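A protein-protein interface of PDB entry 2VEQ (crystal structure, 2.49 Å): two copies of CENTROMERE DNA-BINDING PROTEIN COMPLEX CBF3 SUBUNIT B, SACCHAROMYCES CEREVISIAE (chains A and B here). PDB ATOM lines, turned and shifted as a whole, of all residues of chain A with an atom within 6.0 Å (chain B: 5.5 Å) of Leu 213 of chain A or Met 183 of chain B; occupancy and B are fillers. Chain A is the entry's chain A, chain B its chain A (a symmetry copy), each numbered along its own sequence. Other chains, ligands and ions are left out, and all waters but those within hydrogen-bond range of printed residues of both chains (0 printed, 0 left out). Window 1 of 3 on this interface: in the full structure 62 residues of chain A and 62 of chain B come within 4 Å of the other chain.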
ATOM      1  N   LEU A 174      26.803  28.283 -18.980  1.00  0.00           N
ATOM      2  CA  LEU A 174      26.321  27.616 -17.768  1.00  0.00           C
ATOM      3  C   LEU A 174      25.093  26.771 -18.101  1.00  0.00           C
ATOM      4  O   LEU A 174      24.870  25.706 -17.514  1.00  0.00           O
ATOM      5  CB  LEU A 174      25.953  28.640 -16.685  1.00  0.00           C
ATOM      6  CG  LEU A 174      27.085  29.543 -16.177  1.00  0.00           C
ATOM      7  CD1 LEU A 174      26.535  30.551 -15.190  1.00  0.00           C
ATOM      8  CD2 LEU A 174      28.175  28.701 -15.527  1.00  0.00           C
ATOM      9  N   PHE A 182      25.756  18.547 -14.471  1.00  0.00           N
ATOM     10  CA  PHE A 182      27.116  18.563 -13.938  1.00  0.00           C
ATOM     11  C   PHE A 182      27.277  18.127 -12.491  1.00  0.00           C
ATOM     12  O   PHE A 182      28.331  17.633 -12.111  1.00  0.00           O
ATOM     13  CB  PHE A 182      27.781  19.937 -14.129  1.00  0.00           C
ATOM     14  CG  PHE A 182      27.222  21.025 -13.253  1.00  0.00           C
ATOM     15  CD1 PHE A 182      26.084  21.735 -13.638  1.00  0.00           C
ATOM     16  CD2 PHE A 182      27.857  21.370 -12.061  1.00  0.00           C
ATOM     17  CE1 PHE A 182      25.590  22.777 -12.853  1.00  0.00           C
ATOM     18  CE2 PHE A 182      27.376  22.405 -11.272  1.00  0.00           C
ATOM     19  CZ  PHE A 182      26.236  23.115 -11.668  1.00  0.00           C
ATOM     20  N   MET A 183      26.248  18.296 -11.678  1.00  0.00           N
ATOM     21  CA  MET A 183      26.371  17.883 -10.291  1.00  0.00           C
ATOM     22  C   MET A 183      26.405  16.361 -10.122  1.00  0.00           C
ATOM     23  O   MET A 183      26.929  15.849  -9.132  1.00  0.00           O
ATOM     24  CB  MET A 183      25.244  18.490  -9.457  1.00  0.00           C
ATOM     25  CG  MET A 183      25.367  19.996  -9.301  1.00  0.00           C
ATOM     26  SD  MET A 183      24.440  20.591  -7.898  1.00  0.00           S
ATOM     27  CE  MET A 183      25.748  21.008  -6.786  1.00  0.00           C
ATOM     28  N   LEU A 190      34.304  21.297 -16.134  1.00  0.00           N
ATOM     29  CA  LEU A 190      33.518  22.282 -15.403  1.00  0.00           C
ATOM     30  C   LEU A 190      34.493  23.334 -14.863  1.00  0.00           C
ATOM     31  O   LEU A 190      34.270  24.533 -14.988  1.00  0.00           O
ATOM     32  CB  LEU A 190      32.769  21.625 -14.242  1.00  0.00           C
ATOM     33  CG  LEU A 190      32.230  22.607 -13.197  1.00  0.00           C
ATOM     34  CD1 LEU A 190      31.070  23.386 -13.797  1.00  0.00           C
ATOM     35  CD2 LEU A 190      31.785  21.861 -11.938  1.00  0.00           C
ATOM     36  N   TYR A 194      34.722  27.150 -15.942  1.00  0.00           N
ATOM     37  CA  TYR A 194      34.709  28.220 -14.983  1.00  0.00           C
ATOM     38  C   TYR A 194      35.945  29.080 -15.105  1.00  0.00           C
ATOM     39  O   TYR A 194      35.843  30.314 -14.962  1.00  0.00           O
ATOM     40  CB  TYR A 194      34.535  27.660 -13.543  1.00  0.00           C
ATOM     41  CG  TYR A 194      34.427  28.800 -12.515  1.00  0.00           C
ATOM     42  CD1 TYR A 194      33.196  29.429 -12.325  1.00  0.00           C
ATOM     43  CD2 TYR A 194      35.507  29.289 -11.828  1.00  0.00           C
ATOM     44  CE1 TYR A 194      33.025  30.495 -11.482  1.00  0.00           C
ATOM     45  CE2 TYR A 194      35.354  30.365 -10.952  1.00  0.00           C
ATOM     46  CZ  TYR A 194      34.135  30.975 -10.802  1.00  0.00           C
ATOM     47  OH  TYR A 194      33.959  32.034  -9.948  1.00  0.00           O
ATOM     48  N   PHE A 202      32.567  38.262 -15.049  1.00  0.00           N
ATOM     49  CA  PHE A 202      31.506  37.379 -14.579  1.00  0.00           C
ATOM     50  C   PHE A 202      31.472  37.208 -13.056  1.00  0.00           C
ATOM     51  O   PHE A 202      30.408  37.309 -12.450  1.00  0.00           O
ATOM     52  CB  PHE A 202      31.632  36.001 -15.237  1.00  0.00           C
ATOM     53  CG  PHE A 202      30.696  34.975 -14.664  1.00  0.00           C
ATOM     54  CD1 PHE A 202      29.316  35.096 -14.841  1.00  0.00           C
ATOM     55  CD2 PHE A 202      31.194  33.912 -13.905  1.00  0.00           C
ATOM     56  CE1 PHE A 202      28.438  34.174 -14.265  1.00  0.00           C
ATOM     57  CE2 PHE A 202      30.334  32.986 -13.325  1.00  0.00           C
ATOM     58  CZ  PHE A 202      28.947  33.114 -13.502  1.00  0.00           C
ATOM     59  N   LEU A 208      27.726  35.549  -5.889  1.00  0.00           N
ATOM     60  CA  LEU A 208      27.246  34.358  -5.189  1.00  0.00           C
ATOM     61  C   LEU A 208      27.211  33.132  -6.093  1.00  0.00           C
ATOM     62  O   LEU A 208      27.585  32.031  -5.671  1.00  0.00           O
ATOM     63  CB  LEU A 208      25.856  34.596  -4.597  1.00  0.00           C
ATOM     64  CG  LEU A 208      25.829  35.781  -3.636  1.00  0.00           C
ATOM     65  CD1 LEU A 208      25.200  36.975  -4.350  1.00  0.00           C
ATOM     66  CD2 LEU A 208      25.048  35.437  -2.408  1.00  0.00           C
ATOM     67  N   LEU A 209      26.749  33.321  -7.327  1.00  0.00           N
ATOM     68  CA  LEU A 209      26.694  32.232  -8.285  1.00  0.00           C
ATOM     69  C   LEU A 209      28.123  31.780  -8.540  1.00  0.00           C
ATOM     70  O   LEU A 209      28.414  30.576  -8.523  1.00  0.00           O
ATOM     71  CB  LEU A 209      26.045  32.690  -9.595  1.00  0.00           C
ATOM     72  CG  LEU A 209      26.177  31.773 -10.824  1.00  0.00           C
ATOM     73  CD1 LEU A 209      25.591  30.389 -10.557  1.00  0.00           C
ATOM     74  CD2 LEU A 209      25.462  32.433 -12.008  1.00  0.00           C
ATOM     75  N   ALA A 210      29.019  32.747  -8.753  1.00  0.00           N
ATOM     76  CA  ALA A 210      30.422  32.442  -9.007  1.00  0.00           C
ATOM     77  C   ALA A 210      31.067  31.734  -7.812  1.00  0.00           C
ATOM     78  O   ALA A 210      31.881  30.822  -7.994  1.00  0.00           O
ATOM     79  CB  ALA A 210      31.187  33.717  -9.345  1.00  0.00           C
ATOM     80  N   ASN A 211      30.713  32.141  -6.593  1.00  0.00           N
ATOM     81  CA  ASN A 211      31.268  31.498  -5.413  1.00  0.00           C
ATOM     82  C   ASN A 211      30.743  30.059  -5.271  1.00  0.00           C
ATOM     83  O   ASN A 211      31.455  29.180  -4.770  1.00  0.00           O
ATOM     84  CB  ASN A 211      30.937  32.296  -4.150  1.00  0.00           C
ATOM     85  CG  ASN A 211      31.698  33.613  -4.068  1.00  0.00           C
ATOM     86  OD1 ASN A 211      32.662  33.831  -4.795  1.00  0.00           O
ATOM     87  ND2 ASN A 211      31.273  34.488  -3.160  1.00  0.00           N
ATOM     88  N   SER A 212      29.505  29.818  -5.702  1.00  0.00           N
ATOM     89  CA  SER A 212      28.932  28.472  -5.638  1.00  0.00           C
ATOM     90  C   SER A 212      29.613  27.591  -6.681  1.00  0.00           C
ATOM     91  O   SER A 212      29.931  26.429  -6.417  1.00  0.00           O
ATOM     92  CB  SER A 212      27.421  28.485  -5.914  1.00  0.00           C
ATOM     93  OG  SER A 212      26.698  28.933  -4.785  1.00  0.00           O
ATOM     94  N   LEU A 213      29.815  28.155  -7.866  1.00  0.00           N
ATOM     95  CA  LEU A 213      30.466  27.443  -8.953  1.00  0.00           C
ATOM     96  C   LEU A 213      31.918  27.124  -8.555  1.00  0.00           C
ATOM     97  O   LEU A 213      32.418  26.037  -8.833  1.00  0.00           O
ATOM     98  CB  LEU A 213      30.430  28.298 -10.218  1.00  0.00           C
ATOM     99  CG  LEU A 213      29.464  27.986 -11.372  1.00  0.00           C
ATOM    100  CD1 LEU A 213      28.450  26.905 -11.038  1.00  0.00           C
ATOM    101  CD2 LEU A 213      28.772  29.292 -11.755  1.00  0.00           C
ATOM    102  N   LEU A 214      32.584  28.069  -7.890  1.00  0.00           N
ATOM    103  CA  LEU A 214      33.958  27.855  -7.452  1.00  0.00           C
ATOM    104  C   LEU A 214      33.972  26.707  -6.445  1.00  0.00           C
ATOM    105  O   LEU A 214      34.847  25.845  -6.491  1.00  0.00           O
ATOM    106  CB  LEU A 214      34.536  29.122  -6.810  1.00  0.00           C
ATOM    107  CG  LEU A 214      35.988  29.042  -6.315  1.00  0.00           C
ATOM    108  CD1 LEU A 214      36.924  28.601  -7.446  1.00  0.00           C
ATOM    109  CD2 LEU A 214      36.408  30.408  -5.801  1.00  0.00           C
ATOM    110  N   THR A 215      33.001  26.701  -5.539  1.00  0.00           N
ATOM    111  CA  THR A 215      32.903  25.629  -4.554  1.00  0.00           C
ATOM    112  C   THR A 215      32.754  24.282  -5.273  1.00  0.00           C
ATOM    113  O   THR A 215      33.343  23.287  -4.853  1.00  0.00           O
ATOM    114  CB  THR A 215      31.709  25.857  -3.600  1.00  0.00           C
ATOM    115  OG1 THR A 215      31.987  26.981  -2.767  1.00  0.00           O
ATOM    116  CG2 THR A 215      31.463  24.635  -2.722  1.00  0.00           C
ATOM    117  N   GLN A 216      31.974  24.253  -6.353  1.00  0.00           N
ATOM    118  CA  GLN A 216      31.811  23.027  -7.131  1.00  0.00           C
ATOM    119  C   GLN A 216      33.123  22.636  -7.804  1.00  0.00           C
ATOM    120  O   GLN A 216      33.397  21.446  -7.967  1.00  0.00           O
ATOM    121  CB  GLN A 216      30.734  23.180  -8.208  1.00  0.00           C
ATOM    122  CG  GLN A 216      29.324  22.972  -7.692  1.00  0.00           C
ATOM    123  CD  GLN A 216      29.133  21.598  -7.073  1.00  0.00           C
ATOM    124  OE1 GLN A 216      28.712  21.485  -5.922  1.00  0.00           O
ATOM    125  NE2 GLN A 216      29.440  20.544  -7.839  1.00  0.00           N
ATOM    126  N   CYS A 217      33.925  23.624  -8.208  1.00  0.00           N
ATOM    127  CA  CYS A 217      35.208  23.326  -8.842  1.00  0.00           C
ATOM    128  C   CYS A 217      36.166  22.753  -7.795  1.00  0.00           C
ATOM    129  O   CYS A 217      36.953  21.859  -8.092  1.00  0.00           O
ATOM    130  CB  CYS A 217      35.828  24.582  -9.482  1.00  0.00           C
ATOM    131  SG  CYS A 217      34.901  25.274 -10.881  1.00  0.00           S
ATOM    132  N   ILE A 218      36.093  23.270  -6.570  1.00  0.00           N
ATOM    133  CA  ILE A 218      36.949  22.787  -5.494  1.00  0.00           C
ATOM    134  C   ILE A 218      36.570  21.337  -5.214  1.00  0.00           C
ATOM    135  O   ILE A 218      37.432  20.493  -5.014  1.00  0.00           O
ATOM    136  CB  ILE A 218      36.783  23.640  -4.212  1.00  0.00           C
ATOM    137  CG1 ILE A 218      37.389  25.030  -4.429  1.00  0.00           C
ATOM    138  CG2 ILE A 218      37.472  22.963  -3.037  1.00  0.00           C
ATOM    139  CD1 ILE A 218      37.086  26.009  -3.285  1.00  0.00           C
ATOM    140  N   TYR B 115      11.203  28.371  -3.474  1.00  0.00           N
ATOM    141  CA  TYR B 115      11.968  27.659  -2.460  1.00  0.00           C
ATOM    142  C   TYR B 115      11.003  26.901  -1.554  1.00  0.00           C
ATOM    143  O   TYR B 115      11.269  25.757  -1.190  1.00  0.00           O
ATOM    144  CB  TYR B 115      12.837  28.624  -1.638  1.00  0.00           C
ATOM    145  CG  TYR B 115      14.299  28.641  -2.048  1.00  0.00           C
ATOM    146  CD1 TYR B 115      15.089  27.496  -1.935  1.00  0.00           C
ATOM    147  CD2 TYR B 115      14.893  29.801  -2.549  1.00  0.00           C
ATOM    148  CE1 TYR B 115      16.435  27.500  -2.310  1.00  0.00           C
ATOM    149  CE2 TYR B 115      16.230  29.822  -2.923  1.00  0.00           C
ATOM    150  CZ  TYR B 115      16.998  28.665  -2.803  1.00  0.00           C
ATOM    151  OH  TYR B 115      18.321  28.679  -3.191  1.00  0.00           O
ATOM    152  N   ASP B 181      17.413  29.036  -9.188  1.00  0.00           N
ATOM    153  CA  ASP B 181      18.793  29.432  -9.505  1.00  0.00           C
ATOM    154  C   ASP B 181      19.456  29.396  -8.121  1.00  0.00           C
ATOM    155  O   ASP B 181      20.093  30.359  -7.694  1.00  0.00           O
ATOM    156  CB  ASP B 181      18.880  30.857 -10.078  1.00  0.00           C
ATOM    157  CG  ASP B 181      18.630  30.912 -11.581  1.00  0.00           C
ATOM    158  OD1 ASP B 181      18.956  29.930 -12.287  1.00  0.00           O
ATOM    159  OD2 ASP B 181      18.121  31.949 -12.063  1.00  0.00           O
ATOM    160  N   PHE B 182      19.280  28.282  -7.416  1.00  0.00           N
ATOM    161  CA  PHE B 182      19.808  28.153  -6.059  1.00  0.00           C
ATOM    162  C   PHE B 182      21.278  28.490  -5.874  1.00  0.00           C
ATOM    163  O   PHE B 182      21.685  28.896  -4.793  1.00  0.00           O
ATOM    164  CB  PHE B 182      19.533  26.755  -5.478  1.00  0.00           C
ATOM    165  CG  PHE B 182      20.344  25.652  -6.103  1.00  0.00           C
ATOM    166  CD1 PHE B 182      19.920  25.036  -7.280  1.00  0.00           C
ATOM    167  CD2 PHE B 182      21.512  25.199  -5.490  1.00  0.00           C
ATOM    168  CE1 PHE B 182      20.643  23.980  -7.837  1.00  0.00           C
ATOM    169  CE2 PHE B 182      22.238  24.149  -6.034  1.00  0.00           C
ATOM    170  CZ  PHE B 182      21.803  23.533  -7.213  1.00  0.00           C
ATOM    171  N   MET B 183      22.082  28.335  -6.912  1.00  0.00           N
ATOM    172  CA  MET B 183      23.491  28.655  -6.766  1.00  0.00           C
ATOM    173  C   MET B 183      23.751  30.160  -6.642  1.00  0.00           C
ATOM    174  O   MET B 183      24.768  30.580  -6.088  1.00  0.00           O
ATOM    175  CB  MET B 183      24.290  28.069  -7.929  1.00  0.00           C
ATOM    176  CG  MET B 183      24.355  26.552  -7.896  1.00  0.00           C
ATOM    177  SD  MET B 183      25.722  25.930  -8.858  1.00  0.00           S
ATOM    178  CE  MET B 183      26.804  25.369  -7.579  1.00  0.00           C
ATOM    179  N   ALA B 184      22.819  30.970  -7.133  1.00  0.00           N
ATOM    180  CA  ALA B 184      22.969  32.420  -7.062  1.00  0.00           C
ATOM    181  C   ALA B 184      22.209  32.985  -5.877  1.00  0.00           C
ATOM    182  O   ALA B 184      22.301  34.177  -5.585  1.00  0.00           O
ATOM    183  CB  ALA B 184      22.462  33.063  -8.350  1.00  0.00           C
ATOM    184  N   HIS B 185      21.464  32.119  -5.195  1.00  0.00           N
ATOM    185  CA  HIS B 185      20.647  32.525  -4.056  1.00  0.00           C
ATOM    186  C   HIS B 185      20.720  31.524  -2.905  1.00  0.00           C
ATOM    187  O   HIS B 185      19.799  30.740  -2.689  1.00  0.00           O
ATOM    188  CB  HIS B 185      19.188  32.678  -4.499  1.00  0.00           C
ATOM    189  CG  HIS B 185      19.011  33.569  -5.690  1.00  0.00           C
ATOM    190  ND1 HIS B 185      18.465  33.127  -6.875  1.00  0.00           N
ATOM    191  CD2 HIS B 185      19.351  34.864  -5.892  1.00  0.00           C
ATOM    192  CE1 HIS B 185      18.483  34.109  -7.759  1.00  0.00           C
ATOM    193  NE2 HIS B 185      19.016  35.175  -7.187  1.00  0.00           N
ATOM    194  N   PRO B 186      21.817  31.544  -2.145  1.00  0.00           N
ATOM    195  CA  PRO B 186      21.933  30.606  -1.027  1.00  0.00           C
ATOM    196  C   PRO B 186      20.814  30.820  -0.016  1.00  0.00           C
ATOM    197  O   PRO B 186      20.622  31.924   0.487  1.00  0.00           O
ATOM    198  CB  PRO B 186      23.318  30.917  -0.462  1.00  0.00           C
ATOM    199  CG  PRO B 186      23.493  32.380  -0.782  1.00  0.00           C
ATOM    200  CD  PRO B 186      22.974  32.454  -2.201  1.00  0.00           C
ATOM    201  N   GLN B 216      27.026  21.736  -1.560  1.00  0.00           N
ATOM    202  CA  GLN B 216      26.323  23.014  -1.648  1.00  0.00           C
ATOM    203  C   GLN B 216      25.671  23.366  -0.314  1.00  0.00           C
ATOM    204  O   GLN B 216      25.579  24.545   0.031  1.00  0.00           O
ATOM    205  CB  GLN B 216      25.241  22.991  -2.731  1.00  0.00           C
ATOM    206  CG  GLN B 216      25.773  23.252  -4.127  1.00  0.00           C
ATOM    207  CD  GLN B 216      26.473  24.596  -4.236  1.00  0.00           C
ATOM    208  OE1 GLN B 216      27.630  24.664  -4.650  1.00  0.00           O
ATOM    209  NE2 GLN B 216      25.771  25.674  -3.865  1.00  0.00           N
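The side-chain hydroxyl of Ser 212 of chain A is in hydrogen-bond range of the backbone carbonyl oxygen of Met 183 of chain B, at 2.9 Å.
The backbone carbonyl oxygen (O) of Leu 208 of chain A sits close to the backbone carbonyl oxygen (O) of Met 183 of chain B (3.2 Å).
O of Ser 212 of chain A lies close to OE1 of Gln 216 of chain B (3.4 Å).
The backbone carbonyl oxygen (O) of Leu 213 of chain A lies within hydrogen-bond range of the side-chain sulfur (SG) of Cys 217 of chain A, at 3.3 Å.
O of Leu 208 of chain A is in hydrogen-bond range of OG of Ser 212 of chain A, at 3.3 Å.
CE of Met 183 of chain A touches CG of Gln 216 of chain B, 3.5 Å away.
Leu 208 of chain A touches Ala 184 of chain B.
CD of Pro 186 of chain B touches CD2 of Leu 208 of chain A (3.6 Å).
Leu 209 of chain A touches Met 183 of chain B (CA to O, 3.4 Å).
Ala 184 of chain B touches Leu 209 of chain A (CB to CB, 3.8 Å).
Met 183 of chain B touches Leu 213 of chain A.
Met 183 of chain B touches Gln 216 of chain A.
Gln 216 of chain B touches Gln 216 of chain A (OE1 to OE1, 3.6 Å).
Of chain B, only Met 183 (3.6 Å) comes within 4 Å of Leu 213 of chain A.
Of the printed residues of chain A, Pro 186 of chain B touches Leu 208 (3.6 Å).
Of the printed residues of chain B, Ser 212 of chain A touches Met 183 and Gln 216.
Printed residues of chain B within 4 Å of Leu 209 of chain A: Met 183 (3.4 Å) and Ala 184 (3.8 Å).
Of the printed residues of chain B, Gln 216 of chain A touches Met 183 (3.5 Å) and Gln 216 (3.6 Å).
Of the printed residues of chain B, Leu 208 of chain A touches Met 183, Ala 184 and Pro 186.
The nearest residue of chain B that does not touch Leu 213 of chain A is Gln 216 of chain B (5.2 Å).
The nearest printed residue of chain A that does not touch Met 183 of chain B is Phe 182 of chain A (4.01 Å).
The nearest printed residue of chain B that does not touch Met 183 of chain A is Phe 182 of chain B (4.01 Å).
Printed residues of chain A that touch a printed residue of chain B: Met 183, Leu 208, Leu 209, Ser 212, Leu 213 and Gln 216.
Hydrophobic or aromatic side chains of chain A within 4 Å of the printed part of chain B: Met 183, Leu 208, Leu 209 and Leu 213.
Hydrophobic or aromatic side chains of chain B that line the printed part of chain A: Met 183, Ala 184 and Pro 186.
Met 183 of chain A touches Gln 216 of chain B, and with the chains exchanged Gln 216 of chain A touches Met 183 of chain B.
Gln 216 of chain B touches its own counterpart, Gln 216 of chain A.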
